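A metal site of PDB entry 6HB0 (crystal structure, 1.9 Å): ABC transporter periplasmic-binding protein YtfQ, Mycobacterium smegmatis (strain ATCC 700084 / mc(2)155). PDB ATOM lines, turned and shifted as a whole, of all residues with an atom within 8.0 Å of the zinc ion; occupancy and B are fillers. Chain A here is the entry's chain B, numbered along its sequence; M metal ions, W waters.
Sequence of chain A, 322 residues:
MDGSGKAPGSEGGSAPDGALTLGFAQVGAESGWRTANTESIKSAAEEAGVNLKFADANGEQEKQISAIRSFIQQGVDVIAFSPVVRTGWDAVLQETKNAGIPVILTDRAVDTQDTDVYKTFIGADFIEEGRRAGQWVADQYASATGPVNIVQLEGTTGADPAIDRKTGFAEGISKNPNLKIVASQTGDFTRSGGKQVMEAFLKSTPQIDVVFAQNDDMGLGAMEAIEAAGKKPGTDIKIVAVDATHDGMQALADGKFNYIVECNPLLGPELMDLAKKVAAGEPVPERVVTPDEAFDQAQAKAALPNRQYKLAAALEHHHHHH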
ATOM      1  N   GLY A 123      25.091 -28.075   8.424  1.00  0.00           N
ATOM      2  CA  GLY A 123      26.128 -28.797   9.168  1.00  0.00           C
ATOM      3  C   GLY A 123      25.778 -28.830  10.645  1.00  0.00           C
ATOM      4  O   GLY A 123      24.739 -28.291  11.063  1.00  0.00           O
ATOM      5  N   ALA A 124      26.612 -29.522  11.414  1.00  0.00           N
ATOM      6  CA  ALA A 124      26.360 -29.657  12.832  1.00  0.00           C
ATOM      7  C   ALA A 124      26.665 -28.308  13.459  1.00  0.00           C
ATOM      8  O   ALA A 124      27.551 -27.609  13.013  1.00  0.00           O
ATOM      9  CB  ALA A 124      27.223 -30.738  13.425  1.00  0.00           C
ATOM     10  N   ASP A 125      25.920 -27.998  14.489  1.00  0.00           N
ATOM     11  CA  ASP A 125      26.145 -26.864  15.387  1.00  0.00           C
ATOM     12  C   ASP A 125      26.890 -27.320  16.672  1.00  0.00           C
ATOM     13  O   ASP A 125      26.286 -27.838  17.586  1.00  0.00           O
ATOM     14  CB  ASP A 125      24.792 -26.328  15.768  1.00  0.00           C
ATOM     15  CG  ASP A 125      24.868 -25.013  16.577  1.00  0.00           C
ATOM     16  OD1 ASP A 125      25.971 -24.622  17.076  1.00  0.00           O
ATOM     17  OD2 ASP A 125      23.791 -24.398  16.665  1.00  0.00           O
ATOM     18  N   PHE A 126      28.194 -27.128  16.693  1.00  0.00           N
ATOM     19  CA  PHE A 126      29.035 -27.637  17.737  1.00  0.00           C
ATOM     20  C   PHE A 126      28.836 -26.837  19.044  1.00  0.00           C
ATOM     21  O   PHE A 126      28.979 -27.389  20.097  1.00  0.00           O
ATOM     22  CB  PHE A 126      30.488 -27.534  17.315  1.00  0.00           C
ATOM     23  CG  PHE A 126      30.801 -28.247  16.030  1.00  0.00           C
ATOM     24  CD1 PHE A 126      30.475 -29.570  15.867  1.00  0.00           C
ATOM     25  CD2 PHE A 126      31.440 -27.566  14.971  1.00  0.00           C
ATOM     26  CE1 PHE A 126      30.774 -30.242  14.684  1.00  0.00           C
ATOM     27  CE2 PHE A 126      31.711 -28.219  13.763  1.00  0.00           C
ATOM     28  CZ  PHE A 126      31.379 -29.554  13.635  1.00  0.00           C
ATOM     29  N   ILE A 127      28.508 -25.557  18.955  1.00  0.00           N
ATOM     30  CA  ILE A 127      28.172 -24.760  20.173  1.00  0.00           C
ATOM     31  C   ILE A 127      26.977 -25.374  20.826  1.00  0.00           C
ATOM     32  O   ILE A 127      26.968 -25.635  22.023  1.00  0.00           O
ATOM     33  CB  ILE A 127      27.909 -23.279  19.869  1.00  0.00           C
ATOM     34  CG1 ILE A 127      29.184 -22.657  19.310  1.00  0.00           C
ATOM     35  CG2 ILE A 127      27.387 -22.579  21.127  1.00  0.00           C
ATOM     36  CD1 ILE A 127      29.176 -21.135  19.145  1.00  0.00           C
ATOM     37  N   GLU A 128      25.970 -25.670  20.048  1.00  0.00           N
ATOM     38  CA  GLU A 128      24.747 -26.258  20.564  1.00  0.00           C
ATOM     39  C   GLU A 128      25.031 -27.604  21.209  1.00  0.00           C
ATOM     40  O   GLU A 128      24.451 -27.940  22.230  1.00  0.00           O
ATOM     41  CB  GLU A 128      23.736 -26.409  19.430  1.00  0.00           C
ATOM     42  CG  GLU A 128      22.447 -27.087  19.766  1.00  0.00           C
ATOM     43  CD  GLU A 128      22.243 -28.278  18.848  1.00  0.00           C
ATOM     44  OE1 GLU A 128      21.639 -28.104  17.784  1.00  0.00           O
ATOM     45  OE2 GLU A 128      22.695 -29.390  19.184  1.00  0.00           O
ATOM     46  N   GLU A 129      25.943 -28.400  20.640  1.00  0.00           N
ATOM     47  CA  GLU A 129      26.312 -29.694  21.288  1.00  0.00           C
ATOM     48  C   GLU A 129      26.860 -29.469  22.669  1.00  0.00           C
ATOM     49  O   GLU A 129      26.456 -30.127  23.607  1.00  0.00           O
ATOM     50  CB  GLU A 129      27.392 -30.481  20.498  1.00  0.00           C
ATOM     51  CG  GLU A 129      26.869 -31.104  19.238  1.00  0.00           C
ATOM     52  CD  GLU A 129      27.917 -31.863  18.409  1.00  0.00           C
ATOM     53  OE1 GLU A 129      29.022 -31.321  18.247  1.00  0.00           O
ATOM     54  OE2 GLU A 129      27.593 -32.982  17.872  1.00  0.00           O
ATOM     55  N   ARG A 131      26.501 -26.851  24.519  1.00  0.00           N
ATOM     56  CA  ARG A 131      25.446 -26.341  25.366  1.00  0.00           C
ATOM     57  C   ARG A 131      24.528 -27.394  25.915  1.00  0.00           C
ATOM     58  O   ARG A 131      24.148 -27.360  27.089  1.00  0.00           O
ATOM     59  CB  ARG A 131      24.611 -25.287  24.615  1.00  0.00           C
ATOM     60  CG  ARG A 131      23.598 -24.585  25.506  1.00  0.00           C
ATOM     61  CD  ARG A 131      23.112 -23.307  24.854  1.00  0.00           C
ATOM     62  NE  ARG A 131      22.410 -23.692  23.695  1.00  0.00           N
ATOM     63  CZ  ARG A 131      22.609 -23.303  22.449  1.00  0.00           C
ATOM     64  NH1 ARG A 131      23.404 -22.318  22.098  1.00  0.00           N
ATOM     65  NH2 ARG A 131      21.857 -23.905  21.569  1.00  0.00           N
ATOM     66  N   ARG A 132      24.122 -28.330  25.087  1.00  0.00           N
ATOM     67  CA  ARG A 132      23.264 -29.399  25.580  1.00  0.00           C
ATOM     68  C   ARG A 132      23.991 -30.325  26.586  1.00  0.00           C
ATOM     69  O   ARG A 132      23.393 -30.800  27.553  1.00  0.00           O
ATOM     70  CB  ARG A 132      22.661 -30.158  24.401  1.00  0.00           C
ATOM     71  CG  ARG A 132      21.720 -29.308  23.529  1.00  0.00           C
ATOM     72  CD  ARG A 132      21.651 -29.801  22.059  1.00  0.00           C
ATOM     73  NE  ARG A 132      21.284 -31.155  22.124  1.00  0.00           N
ATOM     74  CZ  ARG A 132      21.682 -32.173  21.390  1.00  0.00           C
ATOM     75  NH1 ARG A 132      22.431 -32.061  20.304  1.00  0.00           N
ATOM     76  NH2 ARG A 132      21.237 -33.341  21.774  1.00  0.00           N
ATOM     77  N   GLU A 262      24.541 -35.429  20.437  1.00  0.00           N
ATOM     78  CA  GLU A 262      25.122 -35.231  19.105  1.00  0.00           C
ATOM     79  C   GLU A 262      24.247 -34.309  18.334  1.00  0.00           C
ATOM     80  O   GLU A 262      23.066 -34.376  18.465  1.00  0.00           O
ATOM     81  CB  GLU A 262      25.284 -36.551  18.348  1.00  0.00           C
ATOM     82  CG  GLU A 262      25.998 -36.341  17.034  1.00  0.00           C
ATOM     83  CD  GLU A 262      26.246 -37.612  16.218  1.00  0.00           C
ATOM     84  OE1 GLU A 262      26.413 -38.712  16.780  1.00  0.00           O
ATOM     85  OE2 GLU A 262      26.350 -37.453  15.004  1.00  0.00           O
ATOM     86  N   CYS A 263      24.867 -33.408  17.564  1.00  0.00           N
ATOM     87  CA  CYS A 263      24.164 -32.624  16.569  1.00  0.00           C
ATOM     88  C   CYS A 263      24.586 -33.246  15.260  1.00  0.00           C
ATOM     89  O   CYS A 263      25.777 -33.314  14.948  1.00  0.00           O
ATOM     90  CB  CYS A 263      24.578 -31.162  16.632  1.00  0.00           C
ATOM     91  SG  CYS A 263      23.670 -30.152  15.441  1.00  0.00           S
ATOM     92  N   ASN A 264      23.620 -33.739  14.483  1.00  0.00           N
ATOM     93  CA  ASN A 264      23.965 -34.446  13.236  1.00  0.00           C
ATOM     94  C   ASN A 264      24.620 -33.551  12.163  1.00  0.00           C
ATOM     95  O   ASN A 264      24.368 -32.351  12.067  1.00  0.00           O
ATOM     96  CB  ASN A 264      22.712 -35.040  12.583  1.00  0.00           C
ATOM     97  CG  ASN A 264      22.124 -36.237  13.343  1.00  0.00           C
ATOM     98  OD1 ASN A 264      20.987 -36.577  13.101  1.00  0.00           O
ATOM     99  ND2 ASN A 264      22.890 -36.873  14.227  1.00  0.00           N
ATOM    100  N   PRO A 265      25.480 -34.134  11.344  1.00  0.00           N
ATOM    101  CA  PRO A 265      25.863 -33.451  10.131  1.00  0.00           C
ATOM    102  C   PRO A 265      24.706 -33.423   9.104  1.00  0.00           C
ATOM    103  O   PRO A 265      23.596 -33.879   9.388  1.00  0.00           O
ATOM    104  CB  PRO A 265      27.014 -34.328   9.630  1.00  0.00           C
ATOM    105  CG  PRO A 265      26.579 -35.686   9.984  1.00  0.00           C
ATOM    106  CD  PRO A 265      25.905 -35.538  11.326  1.00  0.00           C
ATOM    107  N   ARG A 287      20.833 -21.270   8.146  1.00  0.00           N
ATOM    108  CA  ARG A 287      21.409 -22.480   8.688  1.00  0.00           C
ATOM    109  C   ARG A 287      20.308 -23.489   8.870  1.00  0.00           C
ATOM    110  O   ARG A 287      19.325 -23.216   9.513  1.00  0.00           O
ATOM    111  CB  ARG A 287      21.983 -22.183  10.040  1.00  0.00           C
ATOM    112  CG  ARG A 287      23.469 -21.963  10.055  1.00  0.00           C
ATOM    113  CD  ARG A 287      24.066 -23.205  10.689  1.00  0.00           C
ATOM    114  NE  ARG A 287      25.242 -22.919  11.461  1.00  0.00           N
ATOM    115  CZ  ARG A 287      25.937 -23.854  12.069  1.00  0.00           C
ATOM    116  NH1 ARG A 287      26.978 -23.472  12.751  1.00  0.00           N
ATOM    117  NH2 ARG A 287      25.603 -25.164  11.998  1.00  0.00           N
ATOM    118  N   VAL A 288      20.429 -24.626   8.246  1.00  0.00           N
ATOM    119  CA  VAL A 288      19.478 -25.668   8.478  1.00  0.00           C
ATOM    120  C   VAL A 288      19.758 -26.158   9.883  1.00  0.00           C
ATOM    121  O   VAL A 288      20.920 -26.261  10.294  1.00  0.00           O
ATOM    122  CB  VAL A 288      19.698 -26.780   7.469  1.00  0.00           C
ATOM    123  CG1 VAL A 288      18.939 -28.011   7.848  1.00  0.00           C
ATOM    124  CG2 VAL A 288      19.193 -26.342   6.133  1.00  0.00           C
ATOM    125  N   VAL A 289      18.717 -26.494  10.633  1.00  0.00           N
ATOM    126  CA  VAL A 289      18.954 -27.164  11.893  1.00  0.00           C
ATOM    127  C   VAL A 289      18.868 -28.678  11.661  1.00  0.00           C
ATOM    128  O   VAL A 289      17.816 -29.184  11.302  1.00  0.00           O
ATOM    129  CB  VAL A 289      18.001 -26.685  13.006  1.00  0.00           C
ATOM    130  CG1 VAL A 289      18.053 -25.138  13.120  1.00  0.00           C
ATOM    131  CG2 VAL A 289      16.617 -27.206  12.762  1.00  0.00           C
ATOM    132  N   THR A 290      19.988 -29.380  11.821  1.00  0.00           N
ATOM    133  CA  THR A 290      20.032 -30.824  11.609  1.00  0.00           C
ATOM    134  C   THR A 290      19.395 -31.495  12.818  1.00  0.00           C
ATOM    135  O   THR A 290      19.141 -30.829  13.819  1.00  0.00           O
ATOM    136  CB  THR A 290      21.489 -31.313  11.446  1.00  0.00           C
ATOM    137  OG1 THR A 290      22.296 -30.835  12.535  1.00  0.00           O
ATOM    138  CG2 THR A 290      22.058 -30.780  10.137  1.00  0.00           C
ATOM    139  N   PRO A 291      19.080 -32.773  12.729  1.00  0.00           N
ATOM    140  CA  PRO A 291      18.525 -33.443  13.904  1.00  0.00           C
ATOM    141  C   PRO A 291      19.538 -33.609  15.028  1.00  0.00           C
ATOM    142  O   PRO A 291      20.785 -33.683  14.798  1.00  0.00           O
ATOM    143  CB  PRO A 291      18.107 -34.822  13.366  1.00  0.00           C
ATOM    144  CG  PRO A 291      17.961 -34.605  11.915  1.00  0.00           C
ATOM    145  CD  PRO A 291      19.047 -33.642  11.550  1.00  0.00           C
ATOM    146  N   ASP A 292      18.990 -33.639  16.224  1.00  0.00           N
ATOM    147  CA  ASP A 292      19.754 -33.807  17.437  1.00  0.00           C
ATOM    148  C   ASP A 292      19.468 -35.146  18.073  1.00  0.00           C
ATOM    149  O   ASP A 292      18.367 -35.663  18.009  1.00  0.00           O
ATOM    150  CB  ASP A 292      19.408 -32.663  18.391  1.00  0.00           C
ATOM    151  CG  ASP A 292      19.931 -31.355  17.936  1.00  0.00           C
ATOM    152  OD1 ASP A 292      20.983 -31.302  17.243  1.00  0.00           O
ATOM    153  OD2 ASP A 292      19.303 -30.333  18.239  1.00  0.00           O
ATOM    154  N   GLU A 293      20.498 -35.724  18.646  1.00  0.00           N
ATOM    155  CA  GLU A 293      20.426 -36.986  19.354  1.00  0.00           C
ATOM    156  C   GLU A 293      20.862 -36.751  20.801  1.00  0.00           C
ATOM    157  O   GLU A 293      21.715 -35.880  21.049  1.00  0.00           O
ATOM    158  CB  GLU A 293      21.365 -37.973  18.684  1.00  0.00           C
ATOM    159  CG  GLU A 293      20.940 -38.328  17.270  1.00  0.00           C
ATOM    160  CD  GLU A 293      21.781 -39.428  16.602  1.00  0.00           C
ATOM    161  OE1 GLU A 293      22.138 -40.435  17.258  1.00  0.00           O
ATOM    162  OE2 GLU A 293      22.048 -39.306  15.400  1.00  0.00           O
HETATM  163 ZN    ZN M   1      21.842 -29.691  16.520  1.00  0.00          ZN
HETATM  164  O   HOH W   1      20.488 -28.882  15.240  1.00  0.00           O
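NH1 of Arg 132 sits close to OD1 of Asp 292, at 3.5 Å. The side-chain carboxylate of Glu 128 is in salt-bridge range of the guanidinium group of Arg 132 (2.9 Å). The side-chain carboxylate of Asp 125 sits at hydrogen-bond distance from the backbone NH of Glu 128, 3.2 Å away. The side-chain hydroxyl of Thr 290 lies close to the side-chain sulfur of Cys 263. SG of Cys 263 sits close to N of Asp 125, 3.3 Å away. The backbone NH (N) of Cys 263 lies within hydrogen-bond range of the side-chain carboxylate (OE2) of Glu 129, 2.8 Å away. The side-chain hydroxyl (OG1) of Thr 290 lies within hydrogen-bond range of the backbone carbonyl oxygen (O) of Asn 264 (2.6 Å).
The zinc ion is bound by OD1 of Asp 292. Water W1 is bound to the zinc ion. The zinc ion is bound by OE1 of Glu 128. The zinc ion is bound by the side-chain sulfur (SG) of Cys 263. Slightly farther from the zinc ion lies the side-chain carboxylate (OE2) of Glu 128 (2.8 Å).
Residues that only touch the zinc ion: Thr 290. Four residues have an atom within 4 Å of the zinc ion: Glu 128, Cys 263, Thr 290 and Asp 292.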
